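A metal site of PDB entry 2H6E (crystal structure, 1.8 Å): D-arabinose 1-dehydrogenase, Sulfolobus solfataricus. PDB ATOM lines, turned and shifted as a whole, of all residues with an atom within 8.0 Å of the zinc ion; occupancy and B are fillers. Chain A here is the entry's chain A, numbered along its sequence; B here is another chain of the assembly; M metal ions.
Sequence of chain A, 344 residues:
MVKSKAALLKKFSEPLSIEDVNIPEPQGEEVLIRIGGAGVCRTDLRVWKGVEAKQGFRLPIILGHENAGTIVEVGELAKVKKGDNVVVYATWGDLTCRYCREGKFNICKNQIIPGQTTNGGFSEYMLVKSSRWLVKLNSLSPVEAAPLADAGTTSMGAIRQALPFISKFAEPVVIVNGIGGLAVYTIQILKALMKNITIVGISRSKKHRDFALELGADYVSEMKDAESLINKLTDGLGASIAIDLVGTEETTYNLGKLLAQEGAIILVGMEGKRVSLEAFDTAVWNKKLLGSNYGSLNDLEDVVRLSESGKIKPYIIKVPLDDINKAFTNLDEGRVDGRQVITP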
ATOM      1  N   TRP A  92      -2.978  -4.656  -5.630  1.00  0.00           N
ATOM      2  CA  TRP A  92      -4.405  -4.543  -5.873  1.00  0.00           C
ATOM      3  C   TRP A  92      -5.171  -5.480  -4.932  1.00  0.00           C
ATOM      4  O   TRP A  92      -5.322  -6.660  -5.215  1.00  0.00           O
ATOM      5  CB  TRP A  92      -4.728  -4.871  -7.331  1.00  0.00           C
ATOM      6  CG  TRP A  92      -3.948  -4.058  -8.367  1.00  0.00           C
ATOM      7  CD1 TRP A  92      -3.254  -2.902  -8.167  1.00  0.00           C
ATOM      8  CD2 TRP A  92      -3.848  -4.346  -9.763  1.00  0.00           C
ATOM      9  NE1 TRP A  92      -2.712  -2.468  -9.350  1.00  0.00           N
ATOM     10  CE2 TRP A  92      -3.045  -3.337 -10.345  1.00  0.00           C
ATOM     11  CE3 TRP A  92      -4.309  -5.376 -10.572  1.00  0.00           C
ATOM     12  CZ2 TRP A  92      -2.733  -3.328 -11.691  1.00  0.00           C
ATOM     13  CZ3 TRP A  92      -4.010  -5.373 -11.898  1.00  0.00           C
ATOM     14  CH2 TRP A  92      -3.220  -4.360 -12.461  1.00  0.00           C
ATOM     15  N   GLY A  93      -5.655  -4.929  -3.837  1.00  0.00           N
ATOM     16  CA  GLY A  93      -6.408  -5.691  -2.849  1.00  0.00           C
ATOM     17  C   GLY A  93      -7.756  -6.169  -3.341  1.00  0.00           C
ATOM     18  O   GLY A  93      -8.295  -5.660  -4.331  1.00  0.00           O
ATOM     19  N   ASP A  94      -8.327  -7.164  -2.645  1.00  0.00           N
ATOM     20  CA  ASP A  94      -9.615  -7.743  -2.996  1.00  0.00           C
ATOM     21  C   ASP A  94     -10.818  -6.857  -2.627  1.00  0.00           C
ATOM     22  O   ASP A  94     -11.951  -7.158  -3.009  1.00  0.00           O
ATOM     23  CB  ASP A  94      -9.815  -9.139  -2.380  1.00  0.00           C
ATOM     24  CG  ASP A  94      -9.752  -9.157  -0.877  1.00  0.00           C
ATOM     25  OD1 ASP A  94      -9.746  -8.079  -0.237  1.00  0.00           O
ATOM     26  OD2 ASP A  94      -9.661 -10.272  -0.319  1.00  0.00           O
ATOM     27  N   LEU A  95     -10.533  -5.779  -1.884  1.00  0.00           N
ATOM     28  CA  LEU A  95     -11.460  -4.739  -1.503  1.00  0.00           C
ATOM     29  C   LEU A  95     -12.451  -5.156  -0.403  1.00  0.00           C
ATOM     30  O   LEU A  95     -13.196  -4.317   0.097  1.00  0.00           O
ATOM     31  CB  LEU A  95     -12.224  -4.187  -2.717  1.00  0.00           C
ATOM     32  CG  LEU A  95     -11.345  -3.720  -3.870  1.00  0.00           C
ATOM     33  CD1 LEU A  95     -12.185  -3.248  -5.037  1.00  0.00           C
ATOM     34  CD2 LEU A  95     -10.421  -2.600  -3.370  1.00  0.00           C
ATOM     35  N   THR A  96     -12.435  -6.431  -0.013  1.00  0.00           N
ATOM     36  CA  THR A  96     -13.493  -6.996   0.796  1.00  0.00           C
ATOM     37  C   THR A  96     -13.042  -7.219   2.224  1.00  0.00           C
ATOM     38  O   THR A  96     -13.850  -7.152   3.163  1.00  0.00           O
ATOM     39  CB  THR A  96     -14.009  -8.336   0.156  1.00  0.00           C
ATOM     40  OG1 THR A  96     -12.896  -9.212  -0.084  1.00  0.00           O
ATOM     41  CG2 THR A  96     -14.717  -8.065  -1.166  1.00  0.00           C
ATOM     42  N   CYS A  97     -11.749  -7.490   2.401  1.00  0.00           N
ATOM     43  CA  CYS A  97     -11.242  -7.965   3.669  1.00  0.00           C
ATOM     44  C   CYS A  97     -11.080  -6.804   4.635  1.00  0.00           C
ATOM     45  O   CYS A  97     -11.160  -5.618   4.254  1.00  0.00           O
ATOM     46  CB  CYS A  97      -9.908  -8.705   3.452  1.00  0.00           C
ATOM     47  SG  CYS A  97      -8.469  -7.661   3.234  1.00  0.00           S
ATOM     48  N   ARG A  98     -10.848  -7.123   5.903  1.00  0.00           N
ATOM     49  CA  ARG A  98     -10.749  -6.066   6.904  1.00  0.00           C
ATOM     50  C   ARG A  98      -9.508  -5.178   6.759  1.00  0.00           C
ATOM     51  O   ARG A  98      -9.468  -4.075   7.329  1.00  0.00           O
ATOM     52  CB  ARG A  98     -10.840  -6.647   8.313  1.00  0.00           C
ATOM     53  CG  ARG A  98      -9.599  -7.353   8.825  1.00  0.00           C
ATOM     54  CD  ARG A  98      -9.803  -7.759  10.280  1.00  0.00           C
ATOM     55  NE  ARG A  98     -10.185  -6.611  11.118  1.00  0.00           N
ATOM     56  CZ  ARG A  98      -9.351  -5.664  11.531  1.00  0.00           C
ATOM     57  NH1 ARG A  98      -8.052  -5.706  11.224  1.00  0.00           N
ATOM     58  NH2 ARG A  98      -9.800  -4.660  12.274  1.00  0.00           N
ATOM     59  N   TYR A  99      -8.491  -5.639   6.037  1.00  0.00           N
ATOM     60  CA  TYR A  99      -7.322  -4.824   5.751  1.00  0.00           C
ATOM     61  C   TYR A  99      -7.606  -3.835   4.631  1.00  0.00           C
ATOM     62  O   TYR A  99      -7.294  -2.624   4.737  1.00  0.00           O
ATOM     63  CB  TYR A  99      -6.107  -5.716   5.493  1.00  0.00           C
ATOM     64  CG  TYR A  99      -5.799  -6.526   6.723  1.00  0.00           C
ATOM     65  CD1 TYR A  99      -5.107  -5.973   7.790  1.00  0.00           C
ATOM     66  CD2 TYR A  99      -6.246  -7.819   6.837  1.00  0.00           C
ATOM     67  CE1 TYR A  99      -4.853  -6.699   8.938  1.00  0.00           C
ATOM     68  CE2 TYR A  99      -6.015  -8.564   7.990  1.00  0.00           C
ATOM     69  CZ  TYR A  99      -5.301  -8.006   9.032  1.00  0.00           C
ATOM     70  OH  TYR A  99      -5.061  -8.748  10.157  1.00  0.00           O
ATOM     71  N   CYS A 100      -8.252  -4.306   3.567  1.00  0.00           N
ATOM     72  CA  CYS A 100      -8.645  -3.401   2.478  1.00  0.00           C
ATOM     73  C   CYS A 100      -9.641  -2.338   2.962  1.00  0.00           C
ATOM     74  O   CYS A 100      -9.640  -1.190   2.462  1.00  0.00           O
ATOM     75  CB  CYS A 100      -9.254  -4.210   1.330  1.00  0.00           C
ATOM     76  SG  CYS A 100      -8.021  -5.176   0.382  1.00  0.00           S
ATOM     77  N   ARG A 101     -10.491  -2.695   3.924  1.00  0.00           N
ATOM     78  CA  ARG A 101     -11.442  -1.734   4.499  1.00  0.00           C
ATOM     79  C   ARG A 101     -10.800  -0.633   5.355  1.00  0.00           C
ATOM     80  O   ARG A 101     -11.494   0.232   5.880  1.00  0.00           O
ATOM     81  CB  ARG A 101     -12.544  -2.472   5.266  1.00  0.00           C
ATOM     82  CG  ARG A 101     -13.496  -3.187   4.331  1.00  0.00           C
ATOM     83  CD  ARG A 101     -14.451  -4.139   5.019  1.00  0.00           C
ATOM     84  NE  ARG A 101     -15.582  -4.402   4.128  1.00  0.00           N
ATOM     85  CZ  ARG A 101     -16.624  -5.159   4.448  1.00  0.00           C
ATOM     86  NH1 ARG A 101     -16.694  -5.754   5.618  1.00  0.00           N
ATOM     87  NH2 ARG A 101     -17.619  -5.317   3.576  1.00  0.00           N
ATOM     88  N   LYS A 104      -5.454  -0.815   3.619  1.00  0.00           N
ATOM     89  CA  LYS A 104      -4.209  -1.581   3.781  1.00  0.00           C
ATOM     90  C   LYS A 104      -4.127  -2.668   2.700  1.00  0.00           C
ATOM     91  O   LYS A 104      -3.916  -3.861   2.965  1.00  0.00           O
ATOM     92  CB  LYS A 104      -4.049  -2.110   5.204  1.00  0.00           C
ATOM     93  CG  LYS A 104      -4.006  -1.024   6.241  1.00  0.00           C
ATOM     94  CD  LYS A 104      -4.030  -1.576   7.642  1.00  0.00           C
ATOM     95  CE  LYS A 104      -4.176  -0.515   8.695  1.00  0.00           C
ATOM     96  NZ  LYS A 104      -4.399  -1.151  10.038  1.00  0.00           N
ATOM     97  N   PHE A 105      -4.293  -2.210   1.458  1.00  0.00           N
ATOM     98  CA  PHE A 105      -4.282  -3.114   0.282  1.00  0.00           C
ATOM     99  C   PHE A 105      -2.982  -3.898   0.185  1.00  0.00           C
ATOM    100  O   PHE A 105      -2.923  -5.023  -0.341  1.00  0.00           O
ATOM    101  CB  PHE A 105      -4.501  -2.290  -0.977  1.00  0.00           C
ATOM    102  CG  PHE A 105      -5.703  -1.382  -0.916  1.00  0.00           C
ATOM    103  CD1 PHE A 105      -6.985  -1.923  -0.872  1.00  0.00           C
ATOM    104  CD2 PHE A 105      -5.555   0.012  -0.911  1.00  0.00           C
ATOM    105  CE1 PHE A 105      -8.134  -1.110  -0.818  1.00  0.00           C
ATOM    106  CE2 PHE A 105      -6.700   0.857  -0.855  1.00  0.00           C
ATOM    107  CZ  PHE A 105      -7.982   0.306  -0.809  1.00  0.00           C
ATOM    108  N   ASN A 106      -1.926  -3.281   0.690  1.00  0.00           N
ATOM    109  CA  ASN A 106      -0.576  -3.841   0.633  1.00  0.00           C
ATOM    110  C   ASN A 106      -0.397  -5.119   1.469  1.00  0.00           C
ATOM    111  O   ASN A 106       0.556  -5.877   1.243  1.00  0.00           O
ATOM    112  CB  ASN A 106       0.439  -2.755   1.032  1.00  0.00           C
ATOM    113  CG  ASN A 106       0.092  -2.075   2.338  1.00  0.00           C
ATOM    114  OD1 ASN A 106      -1.037  -1.628   2.543  1.00  0.00           O
ATOM    115  ND2 ASN A 106       1.082  -1.954   3.232  1.00  0.00           N
ATOM    116  N   ILE A 107      -1.308  -5.356   2.415  1.00  0.00           N
ATOM    117  CA  ILE A 107      -1.195  -6.560   3.259  1.00  0.00           C
ATOM    118  C   ILE A 107      -2.425  -7.461   3.121  1.00  0.00           C
ATOM    119  O   ILE A 107      -2.656  -8.349   3.944  1.00  0.00           O
ATOM    120  CB  ILE A 107      -0.854  -6.229   4.729  1.00  0.00           C
ATOM    121  CG1 ILE A 107      -1.813  -5.170   5.286  1.00  0.00           C
ATOM    122  CG2 ILE A 107       0.624  -5.763   4.862  1.00  0.00           C
ATOM    123  CD1 ILE A 107      -1.624  -4.884   6.780  1.00  0.00           C
ATOM    124  N   CYS A 108      -3.160  -7.261   2.027  1.00  0.00           N
ATOM    125  CA  CYS A 108      -4.261  -8.146   1.653  1.00  0.00           C
ATOM    126  C   CYS A 108      -3.688  -9.474   1.205  1.00  0.00           C
ATOM    127  O   CYS A 108      -2.784  -9.521   0.360  1.00  0.00           O
ATOM    128  CB  CYS A 108      -5.079  -7.520   0.534  1.00  0.00           C
ATOM    129  SG  CYS A 108      -6.451  -8.569  -0.038  1.00  0.00           S
ATOM    130  N   LYS A 109      -4.221 -10.577   1.741  1.00  0.00           N
ATOM    131  CA  LYS A 109      -3.658 -11.886   1.421  1.00  0.00           C
ATOM    132  C   LYS A 109      -4.178 -12.453   0.078  1.00  0.00           C
ATOM    133  O   LYS A 109      -3.740 -13.507  -0.346  1.00  0.00           O
ATOM    134  CB  LYS A 109      -3.842 -12.853   2.573  1.00  0.00           C
ATOM    135  CG  LYS A 109      -5.250 -13.274   2.914  1.00  0.00           C
ATOM    136  CD  LYS A 109      -5.229 -13.977   4.243  1.00  0.00           C
ATOM    137  CE  LYS A 109      -6.613 -14.457   4.643  1.00  0.00           C
ATOM    138  NZ  LYS A 109      -6.539 -15.307   5.870  1.00  0.00           N
ATOM    139  N   ASN A 110      -5.113 -11.734  -0.545  1.00  0.00           N
ATOM    140  CA  ASN A 110      -5.616 -12.095  -1.885  1.00  0.00           C
ATOM    141  C   ASN A 110      -5.403 -10.947  -2.872  1.00  0.00           C
ATOM    142  O   ASN A 110      -6.243 -10.642  -3.734  1.00  0.00           O
ATOM    143  CB  ASN A 110      -7.083 -12.471  -1.800  1.00  0.00           C
ATOM    144  CG  ASN A 110      -7.307 -13.815  -1.136  1.00  0.00           C
ATOM    145  OD1 ASN A 110      -7.155 -14.852  -1.767  1.00  0.00           O
ATOM    146  ND2 ASN A 110      -7.692 -13.796   0.151  1.00  0.00           N
ATOM    147  N   GLN A 111      -4.249 -10.301  -2.730  1.00  0.00           N
ATOM    148  CA  GLN A 111      -3.886  -9.188  -3.594  1.00  0.00           C
ATOM    149  C   GLN A 111      -3.471  -9.723  -4.979  1.00  0.00           C
ATOM    150  O   GLN A 111      -3.009 -10.876  -5.116  1.00  0.00           O
ATOM    151  CB  GLN A 111      -2.786  -8.331  -2.887  1.00  0.00           C
ATOM    152  CG  GLN A 111      -1.425  -8.921  -2.851  1.00  0.00           C
ATOM    153  CD  GLN A 111      -0.517  -8.297  -1.779  1.00  0.00           C
ATOM    154  OE1 GLN A 111      -0.787  -7.221  -1.255  1.00  0.00           O
ATOM    155  NE2 GLN A 111       0.558  -8.984  -1.461  1.00  0.00           N
ATOM    156  N   GLN B 261      -2.171 -10.626   9.875  1.00  0.00           N
ATOM    157  CA  GLN B 261      -1.426  -9.458   9.405  1.00  0.00           C
ATOM    158  C   GLN B 261      -1.491  -8.338  10.447  1.00  0.00           C
ATOM    159  O   GLN B 261      -2.523  -8.130  11.093  1.00  0.00           O
ATOM    160  CB  GLN B 261      -1.928  -8.893   8.080  1.00  0.00           C
ATOM    161  CG  GLN B 261      -2.008  -9.877   6.902  1.00  0.00           C
ATOM    162  CD  GLN B 261      -3.390 -10.507   6.776  1.00  0.00           C
ATOM    163  OE1 GLN B 261      -3.827 -11.220   7.684  1.00  0.00           O
ATOM    164  NE2 GLN B 261      -4.067 -10.254   5.650  1.00  0.00           N
HETATM  165 ZN    ZN M   1      -8.207  -7.391   0.963  1.00  0.00          ZN
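The backbone carbonyl oxygen (O) of Cys 108 lies close to the side-chain amide oxygen (OE1) of Gln 111, 3.4 Å away.
The side-chain hydroxyl of Thr 96 lies close to the side-chain carboxylate of Asp 94 (3.4 Å).
The side-chain sulfur (SG) of Cys 108 sits close to the backbone NH (N) of Asn 110 (3.5 Å).
The side-chain sulfur (SG) of Cys 97 lies close to the backbone NH (N) of Tyr 99 (3.5 Å).
The side-chain sulfur (SG) of Cys 100 lies close to the backbone NH (N) of Leu 95.
Along chain A the residues within 4 Å of the zinc ion span positions 94 to 108.
The nearest printed residue that does not touch the zinc ion is Leu 95 (4.01 Å).
The zinc ion is bound by the side-chain carboxylate (OD1) of Asp 94 (2.1 Å), the side-chain sulfur (SG) of Cys 100 (2.3 Å), the side-chain sulfur (SG) of Cys 97 (2.3 Å) and the side-chain sulfur (SG) of Cys 108 (2.3 Å).
The zinc ion has four donor atoms within binding distance.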
